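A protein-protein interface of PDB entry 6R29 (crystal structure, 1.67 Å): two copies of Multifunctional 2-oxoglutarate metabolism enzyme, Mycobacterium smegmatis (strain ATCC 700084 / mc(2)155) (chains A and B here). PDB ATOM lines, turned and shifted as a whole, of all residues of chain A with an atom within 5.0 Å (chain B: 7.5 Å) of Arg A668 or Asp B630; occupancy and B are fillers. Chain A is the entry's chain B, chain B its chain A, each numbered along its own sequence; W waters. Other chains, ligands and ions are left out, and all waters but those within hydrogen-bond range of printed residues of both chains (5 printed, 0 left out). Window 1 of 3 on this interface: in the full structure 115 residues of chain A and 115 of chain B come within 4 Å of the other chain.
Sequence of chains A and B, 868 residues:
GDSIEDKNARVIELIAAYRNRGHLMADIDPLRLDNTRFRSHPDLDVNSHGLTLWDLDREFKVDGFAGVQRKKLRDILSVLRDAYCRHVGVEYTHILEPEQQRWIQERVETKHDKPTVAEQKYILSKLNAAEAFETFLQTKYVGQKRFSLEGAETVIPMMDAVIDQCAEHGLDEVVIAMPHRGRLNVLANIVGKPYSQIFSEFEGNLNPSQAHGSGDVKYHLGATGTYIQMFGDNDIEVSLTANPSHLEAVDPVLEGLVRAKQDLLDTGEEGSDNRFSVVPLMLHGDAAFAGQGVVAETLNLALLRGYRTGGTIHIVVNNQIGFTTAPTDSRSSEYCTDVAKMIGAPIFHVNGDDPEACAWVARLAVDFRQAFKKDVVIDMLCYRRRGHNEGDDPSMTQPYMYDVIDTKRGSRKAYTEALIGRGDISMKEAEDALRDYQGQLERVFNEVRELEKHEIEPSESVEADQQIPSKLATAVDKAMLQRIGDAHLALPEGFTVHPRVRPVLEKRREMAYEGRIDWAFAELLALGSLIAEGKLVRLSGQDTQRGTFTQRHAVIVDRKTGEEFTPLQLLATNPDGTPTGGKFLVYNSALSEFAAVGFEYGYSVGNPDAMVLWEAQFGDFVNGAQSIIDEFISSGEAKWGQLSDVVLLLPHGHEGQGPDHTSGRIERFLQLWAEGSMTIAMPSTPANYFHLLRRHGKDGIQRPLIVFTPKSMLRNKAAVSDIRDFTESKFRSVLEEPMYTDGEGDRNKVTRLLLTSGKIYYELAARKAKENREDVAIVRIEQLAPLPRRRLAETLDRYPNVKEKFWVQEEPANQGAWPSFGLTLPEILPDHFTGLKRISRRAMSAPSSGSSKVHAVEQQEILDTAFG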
ATOM      1  N   ASN A 623      24.426 -17.314 -25.813  1.00  0.00           N
ATOM      2  CA  ASN A 623      24.196 -16.011 -25.157  1.00  0.00           C
ATOM      3  C   ASN A 623      23.051 -16.098 -24.086  1.00  0.00           C
ATOM      4  O   ASN A 623      22.975 -15.245 -23.213  1.00  0.00           O
ATOM      5  CB  ASN A 623      23.936 -14.893 -26.165  1.00  0.00           C
ATOM      6  CG  ASN A 623      22.803 -15.144 -27.128  1.00  0.00           C
ATOM      7  OD1 ASN A 623      22.183 -16.223 -27.143  1.00  0.00           O
ATOM      8  ND2 ASN A 623      22.512 -14.133 -27.962  1.00  0.00           N
ATOM      9  N   GLN A 626      24.902 -16.179 -20.887  1.00  0.00           N
ATOM     10  CA  GLN A 626      25.938 -15.145 -20.765  1.00  0.00           C
ATOM     11  C   GLN A 626      26.353 -14.856 -19.328  1.00  0.00           C
ATOM     12  O   GLN A 626      27.560 -14.663 -19.093  1.00  0.00           O
ATOM     13  CB  GLN A 626      25.503 -13.828 -21.440  1.00  0.00           C
ATOM     14  CG  GLN A 626      26.709 -12.912 -21.723  1.00  0.00           C
ATOM     15  CD  GLN A 626      27.554 -13.512 -22.835  1.00  0.00           C
ATOM     16  OE1 GLN A 626      27.053 -13.821 -23.931  1.00  0.00           O
ATOM     17  NE2 GLN A 626      28.842 -13.727 -22.578  1.00  0.00           N
ATOM     18  N   ARG A 665      29.707 -16.413 -31.661  1.00  0.00           N
ATOM     19  CA  ARG A 665      30.276 -15.120 -31.214  1.00  0.00           C
ATOM     20  C   ARG A 665      31.713 -15.301 -30.686  1.00  0.00           C
ATOM     21  O   ARG A 665      32.044 -14.976 -29.530  1.00  0.00           O
ATOM     22  CB  ARG A 665      29.378 -14.389 -30.185  1.00  0.00           C
ATOM     23  CG  ARG A 665      28.006 -14.045 -30.796  1.00  0.00           C
ATOM     24  CD  ARG A 665      27.125 -13.166 -29.934  1.00  0.00           C
ATOM     25  NE  ARG A 665      25.796 -13.064 -30.547  1.00  0.00           N
ATOM     26  CZ  ARG A 665      25.402 -12.077 -31.347  1.00  0.00           C
ATOM     27  NH1 ARG A 665      24.180 -12.084 -31.864  1.00  0.00           N
ATOM     28  NH2 ARG A 665      26.214 -11.063 -31.618  1.00  0.00           N
ATOM     29  N   ILE A 666      32.577 -15.770 -31.579  1.00  0.00           N
ATOM     30  CA  ILE A 666      34.018 -15.928 -31.319  1.00  0.00           C
ATOM     31  C   ILE A 666      34.559 -14.636 -30.711  1.00  0.00           C
ATOM     32  O   ILE A 666      35.327 -14.668 -29.731  1.00  0.00           O
ATOM     33  CB  ILE A 666      34.722 -16.228 -32.684  1.00  0.00           C
ATOM     34  CG1 ILE A 666      34.273 -17.592 -33.236  1.00  0.00           C
ATOM     35  CG2 ILE A 666      36.269 -16.110 -32.573  1.00  0.00           C
ATOM     36  CD1 ILE A 666      34.832 -17.876 -34.666  1.00  0.00           C
ATOM     37  N   GLU A 667      34.178 -13.502 -31.316  1.00  0.00           N
ATOM     38  CA  GLU A 667      34.685 -12.185 -30.915  1.00  0.00           C
ATOM     39  C   GLU A 667      34.407 -11.885 -29.428  1.00  0.00           C
ATOM     40  O   GLU A 667      35.223 -11.219 -28.775  1.00  0.00           O
ATOM     41  CB  GLU A 667      34.105 -11.068 -31.810  1.00  0.00           C
ATOM     42  CG  GLU A 667      32.582 -10.938 -31.807  1.00  0.00           C
ATOM     43  CD  GLU A 667      31.730 -11.977 -32.520  1.00  0.00           C
ATOM     44  OE1 GLU A 667      32.266 -12.843 -33.262  1.00  0.00           O
ATOM     45  OE2 GLU A 667      30.493 -11.897 -32.346  1.00  0.00           O
ATOM     46  N   ARG A 668      33.273 -12.388 -28.903  1.00  0.00           N
ATOM     47  CA  ARG A 668      32.920 -12.128 -27.503  1.00  0.00           C
ATOM     48  C   ARG A 668      33.814 -12.950 -26.570  1.00  0.00           C
ATOM     49  O   ARG A 668      34.307 -12.418 -25.559  1.00  0.00           O
ATOM     50  CB  ARG A 668      31.426 -12.410 -27.272  1.00  0.00           C
ATOM     51  CG  ARG A 668      31.010 -12.001 -25.856  1.00  0.00           C
ATOM     52  CD  ARG A 668      29.484 -12.079 -25.749  1.00  0.00           C
ATOM     53  NE  ARG A 668      28.854 -11.088 -26.622  1.00  0.00           N
ATOM     54  CZ  ARG A 668      27.556 -11.065 -26.907  1.00  0.00           C
ATOM     55  NH1 ARG A 668      26.736 -11.973 -26.380  1.00  0.00           N
ATOM     56  NH2 ARG A 668      27.059 -10.112 -27.692  1.00  0.00           N
ATOM     57  N   PHE A 669      34.040 -14.246 -26.907  1.00  0.00           N
ATOM     58  CA  PHE A 669      34.937 -15.074 -26.097  1.00  0.00           C
ATOM     59  C   PHE A 669      36.379 -14.547 -26.155  1.00  0.00           C
ATOM     60  O   PHE A 669      37.074 -14.553 -25.130  1.00  0.00           O
ATOM     61  CB  PHE A 669      34.895 -16.541 -26.546  1.00  0.00           C
ATOM     62  CG  PHE A 669      33.609 -17.208 -26.124  1.00  0.00           C
ATOM     63  CD1 PHE A 669      33.483 -17.774 -24.853  1.00  0.00           C
ATOM     64  CD2 PHE A 669      32.523 -17.277 -26.997  1.00  0.00           C
ATOM     65  CE1 PHE A 669      32.286 -18.410 -24.460  1.00  0.00           C
ATOM     66  CE2 PHE A 669      31.333 -17.915 -26.616  1.00  0.00           C
ATOM     67  CZ  PHE A 669      31.218 -18.461 -25.338  1.00  0.00           C
ATOM     68  N   LEU A 670      36.830 -14.049 -27.335  1.00  0.00           N
ATOM     69  CA  LEU A 670      38.185 -13.520 -27.418  1.00  0.00           C
ATOM     70  C   LEU A 670      38.329 -12.224 -26.607  1.00  0.00           C
ATOM     71  O   LEU A 670      39.407 -11.950 -26.093  1.00  0.00           O
ATOM     72  CB  LEU A 670      38.588 -13.288 -28.888  1.00  0.00           C
ATOM     73  CG  LEU A 670      38.753 -14.585 -29.698  1.00  0.00           C
ATOM     74  CD1 LEU A 670      39.090 -14.262 -31.167  1.00  0.00           C
ATOM     75  CD2 LEU A 670      39.910 -15.465 -29.127  1.00  0.00           C
ATOM     76  N   GLN A 671      37.230 -11.438 -26.492  1.00  0.00           N
ATOM     77  CA  GLN A 671      37.227 -10.190 -25.711  1.00  0.00           C
ATOM     78  C   GLN A 671      37.284 -10.510 -24.217  1.00  0.00           C
ATOM     79  O   GLN A 671      37.969  -9.830 -23.451  1.00  0.00           O
ATOM     80  CB  GLN A 671      35.942  -9.401 -26.037  1.00  0.00           C
ATOM     81  CG  GLN A 671      35.858  -8.033 -25.380  1.00  0.00           C
ATOM     82  CD  GLN A 671      34.751  -7.264 -26.076  1.00  0.00           C
ATOM     83  OE1 GLN A 671      33.566  -7.436 -25.793  1.00  0.00           O
ATOM     84  NE2 GLN A 671      35.124  -6.438 -27.029  1.00  0.00           N
ATOM     85  N   LEU A 672      36.556 -11.544 -23.803  1.00  0.00           N
ATOM     86  CA  LEU A 672      36.530 -11.967 -22.406  1.00  0.00           C
ATOM     87  C   LEU A 672      37.868 -12.531 -21.975  1.00  0.00           C
ATOM     88  O   LEU A 672      38.230 -12.467 -20.796  1.00  0.00           O
ATOM     89  CB  LEU A 672      35.446 -13.049 -22.208  1.00  0.00           C
ATOM     90  CG  LEU A 672      34.020 -12.504 -22.104  1.00  0.00           C
ATOM     91  CD1 LEU A 672      33.019 -13.623 -22.236  1.00  0.00           C
ATOM     92  CD2 LEU A 672      33.817 -11.803 -20.730  1.00  0.00           C
ATOM     93  N   PRO B 244      13.388 -13.708 -32.840  1.00  0.00           N
ATOM     94  CA  PRO B 244      14.601 -14.462 -33.213  1.00  0.00           C
ATOM     95  C   PRO B 244      14.359 -15.968 -33.009  1.00  0.00           C
ATOM     96  O   PRO B 244      13.267 -16.385 -32.539  1.00  0.00           O
ATOM     97  CB  PRO B 244      15.631 -13.938 -32.212  1.00  0.00           C
ATOM     98  CG  PRO B 244      14.795 -13.738 -30.939  1.00  0.00           C
ATOM     99  CD  PRO B 244      13.459 -13.218 -31.447  1.00  0.00           C
ATOM    100  N   HIS B 246      15.695 -17.716 -30.689  1.00  0.00           N
ATOM    101  CA  HIS B 246      15.726 -17.926 -29.225  1.00  0.00           C
ATOM    102  C   HIS B 246      14.320 -18.081 -28.672  1.00  0.00           C
ATOM    103  O   HIS B 246      13.572 -17.114 -28.574  1.00  0.00           O
ATOM    104  CB  HIS B 246      16.472 -16.783 -28.545  1.00  0.00           C
ATOM    105  CG  HIS B 246      17.912 -16.698 -28.957  1.00  0.00           C
ATOM    106  ND1 HIS B 246      18.279 -16.574 -30.285  1.00  0.00           N
ATOM    107  CD2 HIS B 246      19.028 -16.741 -28.184  1.00  0.00           C
ATOM    108  CE1 HIS B 246      19.617 -16.586 -30.292  1.00  0.00           C
ATOM    109  NE2 HIS B 246      20.109 -16.645 -29.043  1.00  0.00           N
ATOM    110  N   ALA B 625      20.308  -9.858 -19.549  1.00  0.00           N
ATOM    111  CA  ALA B 625      19.383  -9.606 -20.673  1.00  0.00           C
ATOM    112  C   ALA B 625      20.142  -9.723 -22.001  1.00  0.00           C
ATOM    113  O   ALA B 625      19.733  -9.124 -23.009  1.00  0.00           O
ATOM    114  CB  ALA B 625      18.777  -8.204 -20.526  1.00  0.00           C
ATOM    115  N   GLN B 626      21.265 -10.480 -22.012  1.00  0.00           N
ATOM    116  CA  GLN B 626      22.085 -10.541 -23.239  1.00  0.00           C
ATOM    117  C   GLN B 626      21.303 -11.000 -24.456  1.00  0.00           C
ATOM    118  O   GLN B 626      21.521 -10.432 -25.544  1.00  0.00           O
ATOM    119  CB  GLN B 626      23.322 -11.444 -23.038  1.00  0.00           C
ATOM    120  CG  GLN B 626      24.393 -11.188 -24.122  1.00  0.00           C
ATOM    121  CD  GLN B 626      25.025  -9.823 -23.898  1.00  0.00           C
ATOM    122  OE1 GLN B 626      25.519  -9.522 -22.798  1.00  0.00           O
ATOM    123  NE2 GLN B 626      24.995  -8.944 -24.904  1.00  0.00           N
ATOM    124  N   SER B 627      20.391 -11.995 -24.304  1.00  0.00           N
ATOM    125  CA  SER B 627      19.599 -12.433 -25.473  1.00  0.00           C
ATOM    126  C   SER B 627      18.768 -11.272 -26.057  1.00  0.00           C
ATOM    127  O   SER B 627      18.653 -11.167 -27.277  1.00  0.00           O
ATOM    128  CB  SER B 627      18.646 -13.571 -25.084  1.00  0.00           C
ATOM    129  OG  SER B 627      19.363 -14.671 -24.545  1.00  0.00           O
ATOM    130  N   ILE B 628      18.186 -10.397 -25.202  1.00  0.00           N
ATOM    131  CA  ILE B 628      17.405  -9.261 -25.726  1.00  0.00           C
ATOM    132  C   ILE B 628      18.342  -8.263 -26.425  1.00  0.00           C
ATOM    133  O   ILE B 628      18.006  -7.750 -27.491  1.00  0.00           O
ATOM    134  CB  ILE B 628      16.596  -8.561 -24.604  1.00  0.00           C
ATOM    135  CG1 ILE B 628      15.612  -9.571 -23.934  1.00  0.00           C
ATOM    136  CG2 ILE B 628      15.847  -7.328 -25.176  1.00  0.00           C
ATOM    137  CD1 ILE B 628      14.528 -10.184 -24.922  1.00  0.00           C
ATOM    138  N   ILE B 629      19.504  -7.962 -25.805  1.00  0.00           N
ATOM    139  CA  ILE B 629      20.442  -7.032 -26.425  1.00  0.00           C
ATOM    140  C   ILE B 629      20.900  -7.546 -27.782  1.00  0.00           C
ATOM    141  O   ILE B 629      20.892  -6.803 -28.774  1.00  0.00           O
ATOM    142  CB  ILE B 629      21.641  -6.800 -25.478  1.00  0.00           C
ATOM    143  CG1 ILE B 629      21.200  -5.994 -24.237  1.00  0.00           C
ATOM    144  CG2 ILE B 629      22.805  -6.080 -26.237  1.00  0.00           C
ATOM    145  CD1 ILE B 629      22.213  -6.155 -23.079  1.00  0.00           C
ATOM    146  N   ASP B 630      21.327  -8.804 -27.823  1.00  0.00           N
ATOM    147  CA  ASP B 630      21.855  -9.369 -29.061  1.00  0.00           C
ATOM    148  C   ASP B 630      20.805  -9.557 -30.157  1.00  0.00           C
ATOM    149  O   ASP B 630      21.107  -9.319 -31.331  1.00  0.00           O
ATOM    150  CB  ASP B 630      22.469 -10.754 -28.787  1.00  0.00           C
ATOM    151  CG  ASP B 630      23.710 -10.780 -27.910  1.00  0.00           C
ATOM    152  OD1 ASP B 630      24.261  -9.683 -27.610  1.00  0.00           O
ATOM    153  OD2 ASP B 630      24.165 -11.910 -27.551  1.00  0.00           O
ATOM    154  N   GLU B 631      19.630 -10.100 -29.788  1.00  0.00           N
ATOM    155  CA  GLU B 631      18.633 -10.541 -30.763  1.00  0.00           C
ATOM    156  C   GLU B 631      17.575  -9.510 -31.130  1.00  0.00           C
ATOM    157  O   GLU B 631      16.916  -9.685 -32.155  1.00  0.00           O
ATOM    158  CB  GLU B 631      17.927 -11.794 -30.240  1.00  0.00           C
ATOM    159  CG  GLU B 631      18.876 -12.945 -29.931  1.00  0.00           C
ATOM    160  CD  GLU B 631      19.613 -13.470 -31.145  1.00  0.00           C
ATOM    161  OE1 GLU B 631      18.974 -13.568 -32.219  1.00  0.00           O
ATOM    162  OE2 GLU B 631      20.815 -13.803 -31.019  1.00  0.00           O
ATOM    163  N   PHE B 632      17.351  -8.504 -30.265  1.00  0.00           N
ATOM    164  CA  PHE B 632      16.335  -7.491 -30.553  1.00  0.00           C
ATOM    165  C   PHE B 632      16.942  -6.094 -30.652  1.00  0.00           C
ATOM    166  O   PHE B 632      16.832  -5.448 -31.701  1.00  0.00           O
ATOM    167  CB  PHE B 632      15.259  -7.503 -29.434  1.00  0.00           C
ATOM    168  CG  PHE B 632      14.335  -8.691 -29.454  1.00  0.00           C
ATOM    169  CD1 PHE B 632      13.159  -8.667 -30.201  1.00  0.00           C
ATOM    170  CD2 PHE B 632      14.602  -9.811 -28.669  1.00  0.00           C
ATOM    171  CE1 PHE B 632      12.275  -9.750 -30.178  1.00  0.00           C
ATOM    172  CE2 PHE B 632      13.702 -10.897 -28.639  1.00  0.00           C
ATOM    173  CZ  PHE B 632      12.534 -10.834 -29.366  1.00  0.00           C
ATOM    174  N   ILE B 633      17.555  -5.605 -29.578  1.00  0.00           N
ATOM    175  CA  ILE B 633      18.015  -4.207 -29.528  1.00  0.00           C
ATOM    176  C   ILE B 633      19.068  -3.899 -30.582  1.00  0.00           C
ATOM    177  O   ILE B 633      18.914  -2.933 -31.346  1.00  0.00           O
ATOM    178  CB  ILE B 633      18.531  -3.870 -28.100  1.00  0.00           C
ATOM    179  CG1 ILE B 633      17.324  -3.833 -27.112  1.00  0.00           C
ATOM    180  CG2 ILE B 633      19.321  -2.528 -28.045  1.00  0.00           C
ATOM    181  CD1 ILE B 633      17.768  -3.745 -25.620  1.00  0.00           C
ATOM    182  N   SER B 634      20.138  -4.716 -30.625  1.00  0.00           N
ATOM    183  CA  SER B 634      21.237  -4.387 -31.524  1.00  0.00           C
ATOM    184  C   SER B 634      20.981  -4.738 -32.988  1.00  0.00           C
ATOM    185  O   SER B 634      21.707  -4.238 -33.851  1.00  0.00           O
ATOM    186  CB  SER B 634      22.500  -5.119 -31.061  1.00  0.00           C
ATOM    187  OG  SER B 634      22.369  -6.523 -31.249  1.00  0.00           O
ATOM    188  N   SER B 635      19.978  -5.598 -33.272  1.00  0.00           N
ATOM    189  CA  SER B 635      19.840  -6.160 -34.605  1.00  0.00           C
ATOM    190  C   SER B 635      18.432  -6.200 -35.214  1.00  0.00           C
ATOM    191  O   SER B 635      18.318  -6.579 -36.382  1.00  0.00           O
ATOM    192  CB  SER B 635      20.368  -7.599 -34.554  1.00  0.00           C
ATOM    193  OG  SER B 635      19.708  -8.311 -33.514  1.00  0.00           O
ATOM    194  N   GLY B 636      17.384  -5.853 -34.463  1.00  0.00           N
ATOM    195  CA  GLY B 636      16.022  -5.965 -34.992  1.00  0.00           C
ATOM    196  C   GLY B 636      15.738  -5.089 -36.205  1.00  0.00           C
ATOM    197  O   GLY B 636      14.947  -5.476 -37.076  1.00  0.00           O
ATOM    198  N   LYS B 639      17.442  -6.931 -39.191  1.00  0.00           N
ATOM    199  CA  LYS B 639      16.837  -8.234 -39.494  1.00  0.00           C
ATOM    200  C   LYS B 639      15.387  -8.155 -39.958  1.00  0.00           C
ATOM    201  O   LYS B 639      14.977  -8.947 -40.809  1.00  0.00           O
ATOM    202  CB  LYS B 639      16.891  -9.143 -38.257  1.00  0.00           C
ATOM    203  CG  LYS B 639      18.341  -9.544 -37.875  1.00  0.00           C
ATOM    204  CD  LYS B 639      18.399 -10.573 -36.726  1.00  0.00           C
ATOM    205  CE  LYS B 639      17.708 -10.097 -35.451  1.00  0.00           C
ATOM    206  NZ  LYS B 639      18.025 -11.051 -34.336  1.00  0.00           N
ATOM    207  N   TRP B 640      14.585  -7.294 -39.324  1.00  0.00           N
ATOM    208  CA  TRP B 640      13.148  -7.309 -39.558  1.00  0.00           C
ATOM    209  C   TRP B 640      12.548  -5.977 -39.965  1.00  0.00           C
ATOM    210  O   TRP B 640      11.349  -5.955 -40.281  1.00  0.00           O
ATOM    211  CB  TRP B 640      12.418  -7.755 -38.254  1.00  0.00           C
ATOM    212  CG  TRP B 640      12.963  -8.984 -37.586  1.00  0.00           C
ATOM    213  CD1 TRP B 640      13.216 -10.196 -38.165  1.00  0.00           C
ATOM    214  CD2 TRP B 640      13.293  -9.122 -36.199  1.00  0.00           C
ATOM    215  NE1 TRP B 640      13.701 -11.079 -37.217  1.00  0.00           N
ATOM    216  CE2 TRP B 640      13.771 -10.441 -36.008  1.00  0.00           C
ATOM    217  CE3 TRP B 640      13.200  -8.266 -35.083  1.00  0.00           C
ATOM    218  CZ2 TRP B 640      14.178 -10.918 -34.747  1.00  0.00           C
ATOM    219  CZ3 TRP B 640      13.621  -8.731 -33.838  1.00  0.00           C
ATOM    220  CH2 TRP B 640      14.125 -10.033 -33.680  1.00  0.00           C
ATOM    221  N   ARG B 668      31.537  -4.614 -25.111  1.00  0.00           N
ATOM    222  CA  ARG B 668      30.597  -5.546 -25.742  1.00  0.00           C
ATOM    223  C   ARG B 668      29.594  -4.780 -26.612  1.00  0.00           C
ATOM    224  O   ARG B 668      29.304  -5.207 -27.741  1.00  0.00           O
ATOM    225  CB  ARG B 668      29.874  -6.376 -24.673  1.00  0.00           C
ATOM    226  CG  ARG B 668      29.005  -7.467 -25.292  1.00  0.00           C
ATOM    227  CD  ARG B 668      28.518  -8.430 -24.210  1.00  0.00           C
ATOM    228  NE  ARG B 668      29.647  -9.172 -23.634  1.00  0.00           N
ATOM    229  CZ  ARG B 668      29.577  -9.908 -22.533  1.00  0.00           C
ATOM    230  NH1 ARG B 668      28.424 -10.023 -21.871  1.00  0.00           N
ATOM    231  NH2 ARG B 668      30.643 -10.584 -22.109  1.00  0.00           N
ATOM    232  N   PHE B 669      29.081  -3.632 -26.101  1.00  0.00           N
ATOM    233  CA  PHE B 669      28.160  -2.803 -26.903  1.00  0.00           C
ATOM    234  C   PHE B 669      28.880  -2.231 -28.127  1.00  0.00           C
ATOM    235  O   PHE B 669      28.292  -2.184 -29.204  1.00  0.00           O
ATOM    236  CB  PHE B 669      27.549  -1.674 -26.072  1.00  0.00           C
ATOM    237  CG  PHE B 669      26.512  -2.211 -25.106  1.00  0.00           C
ATOM    238  CD1 PHE B 669      25.188  -2.398 -25.514  1.00  0.00           C
ATOM    239  CD2 PHE B 669      26.861  -2.541 -23.796  1.00  0.00           C
ATOM    240  CE1 PHE B 669      24.222  -2.886 -24.614  1.00  0.00           C
ATOM    241  CE2 PHE B 669      25.894  -3.015 -22.888  1.00  0.00           C
ATOM    242  CZ  PHE B 669      24.592  -3.220 -23.316  1.00  0.00           C
ATOM    243  N   GLN B 671      31.324  -3.643 -29.748  1.00  0.00           N
ATOM    244  CA  GLN B 671      31.535  -4.786 -30.655  1.00  0.00           C
ATOM    245  C   GLN B 671      30.240  -5.098 -31.402  1.00  0.00           C
ATOM    246  O   GLN B 671      30.270  -5.408 -32.591  1.00  0.00           O
ATOM    247  CB  GLN B 671      31.979  -6.008 -29.823  1.00  0.00           C
ATOM    248  CG  GLN B 671      32.272  -7.277 -30.621  1.00  0.00           C
ATOM    249  CD  GLN B 671      33.027  -8.215 -29.696  1.00  0.00           C
ATOM    250  OE1 GLN B 671      32.432  -8.957 -28.909  1.00  0.00           O
ATOM    251  NE2 GLN B 671      34.339  -8.156 -29.739  1.00  0.00           N
ATOM    252  N   LEU B 672      29.097  -5.032 -30.694  1.00  0.00           N
ATOM    253  CA  LEU B 672      27.792  -5.294 -31.302  1.00  0.00           C
ATOM    254  C   LEU B 672      27.429  -4.219 -32.310  1.00  0.00           C
ATOM    255  O   LEU B 672      26.710  -4.488 -33.275  1.00  0.00           O
ATOM    256  CB  LEU B 672      26.709  -5.324 -30.208  1.00  0.00           C
ATOM    257  CG  LEU B 672      26.627  -6.635 -29.435  1.00  0.00           C
ATOM    258  CD1 LEU B 672      25.774  -6.461 -28.203  1.00  0.00           C
ATOM    259  CD2 LEU B 672      26.020  -7.765 -30.329  1.00  0.00           C
HETATM  260  O   HOH W   1      37.166  -9.643 -29.885  1.00  0.00           O
HETATM  261  O   HOH W   2      29.640  -9.240 -28.680  1.00  0.00           O
HETATM  262  O   HOH W   3      23.272  -9.472 -33.149  1.00  0.00           O
HETATM  263  O   HOH W   4      32.580  -9.205 -23.884  1.00  0.00           O
HETATM  264  O   HOH W   5      22.107 -13.735 -33.464  1.00  0.00           O
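A ring nitrogen (NE2) of His B246 sits at hydrogen-bond distance from the side-chain amide oxygen of Asn A623, at 2.8 Å.
The side-chain amide nitrogen (ND2) of Asn A623 sits at hydrogen-bond distance from the side-chain carboxylate (OD2) of Asp B630 (2.8 Å).
The guanidinium group (NE) of Arg A665 is in salt-bridge range of the side-chain carboxylate (OD2) of Asp B630 (3.6 Å).
OD2 of Asp B630 is in salt-bridge range of NH1 of Arg A668 (2.8 Å).
NH1 of Arg A665 lies within salt-bridge range of OE2 of Glu B631, at 3.9 Å.
The side-chain amide nitrogen (NE2) of Gln B671 is in hydrogen-bond range of the backbone carbonyl oxygen (O) of Glu A667.
The side-chain amide nitrogen of Gln B671 lies close to the side-chain amide nitrogen of Gln A671 (3.3 Å).
The side-chain carboxylate (OD1) of Asp B630 sits at hydrogen-bond distance from the side-chain amide nitrogen (NE2) of Gln B626 (2.9 Å).
The side-chain amide oxygen (OE1) of Gln B626 lies within hydrogen-bond range of the guanidinium group (NH1) of Arg B668 (3.1 Å).
The side-chain hydroxyl of Ser B634 sits at hydrogen-bond distance from the backbone carbonyl oxygen of Asp B630, 3.1 Å away.
The backbone carbonyl oxygen (O) of Asp B630 sits at hydrogen-bond distance from the side-chain hydroxyl (OG) of Ser B635 (2.8 Å).
O of Glu B631 sits at hydrogen-bond distance from OG of Ser B635, at 3.4 Å.
OE1 of Glu B631 lies within salt-bridge range of NZ of Lys B639 (3.4 Å).
Among the printed residues, pairs that only touch across the chains: Arg A668 with Gln B626, Gln A626 with Arg B668, Arg A668 with Gln B671, Asn A623 with Glu B631, Gln A671 with Arg B668, Arg A665 with Leu B672, Arg A668 with Arg B668, Gln A626 with Gln B626, Leu A672 with Arg B668, Arg A668 with Leu B672, Asn A623 with Gln B626 and Asn A623 with Ser B627.
Of the 10 printed residues of chain A, 7 touch a printed residue of chain B.
Hydrophobic or aromatic side chains of chain A within 4 Å of the printed part of chain B: Leu A672.
Along chain B the printed residues that touch a printed residue of chain A span positions 246 to 672.
Among the printed residues, 19 pairs touch across the chains.
Among the printed residues, Asp or Glu carboxylates within 4 Å of a Lys or Arg side-chain nitrogen of the other chain: Arg A665 with Asp B630 (3.6 Å), Arg A665 with Glu B631 (3.9 Å) and Arg A668 with Asp B630 (2.8 Å).
Water W1 bridges O of Glu A667 and NE2 of Gln B671.
Water W5 lies within hydrogen-bond range of the side-chain carboxylate of Glu B631 (2.8 Å) and the guanidinium group of Arg A665 (3.1 Å).
Water W4 lies within hydrogen-bond range of OE1 of Gln A671 and NE of Arg B668.
Water W2 lies within hydrogen-bond range of the side-chain amide oxygen (OE1) of Gln B671 (2.8 Å) and the guanidinium group (NE) of Arg A668 (2.9 Å).
Water W3 lies within hydrogen-bond range of the backbone carbonyl oxygen of Asp B630 and the guanidinium group of Arg A665.
Of chain B, only Gln B626 (3.3 Å), Asp B630 (2.8 Å), Arg B668 (3.6 Å), Gln B671 (3.5 Å) and Leu B672 (3.7 Å) come within 4 Å of Arg A668.
Of the printed residues of chain A, Asp B630 touches Asn A623 (2.8 Å), Arg A665 (3.6 Å) and Arg A668 (2.8 Å).
Printed residues of chain B within 4 Å of Gln A671: Arg B668 (3.5 Å) and Gln B671 (3.3 Å).
Of the printed residues of chain B, Arg A665 touches Asp B630, Glu B631 and Leu B672.
Printed residues of chain A within 4 Å of Glu B631: Asn A623 (3.5 Å) and Arg A665 (3.9 Å).
Of the printed residues of chain A, Ser B627 touches Asn A623 (3.9 Å).
The nearest printed residue of chain A that does not touch Asp B630 is Gln A626 (5.0 Å).
The nearest printed residue of chain A that does not touch His B246 is Arg A665 (6.6 Å).
Gln A626 touches Arg B668, and with the chains exchanged Arg A668 touches Gln B626.
Arg A668 touches Gln B671, and with the chains exchanged Gln A671 touches Arg B668.
Arg A668 touches Leu B672, and with the chains exchanged Leu A672 touches Arg B668.
Gln A671 touches its own counterpart, Gln B671.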
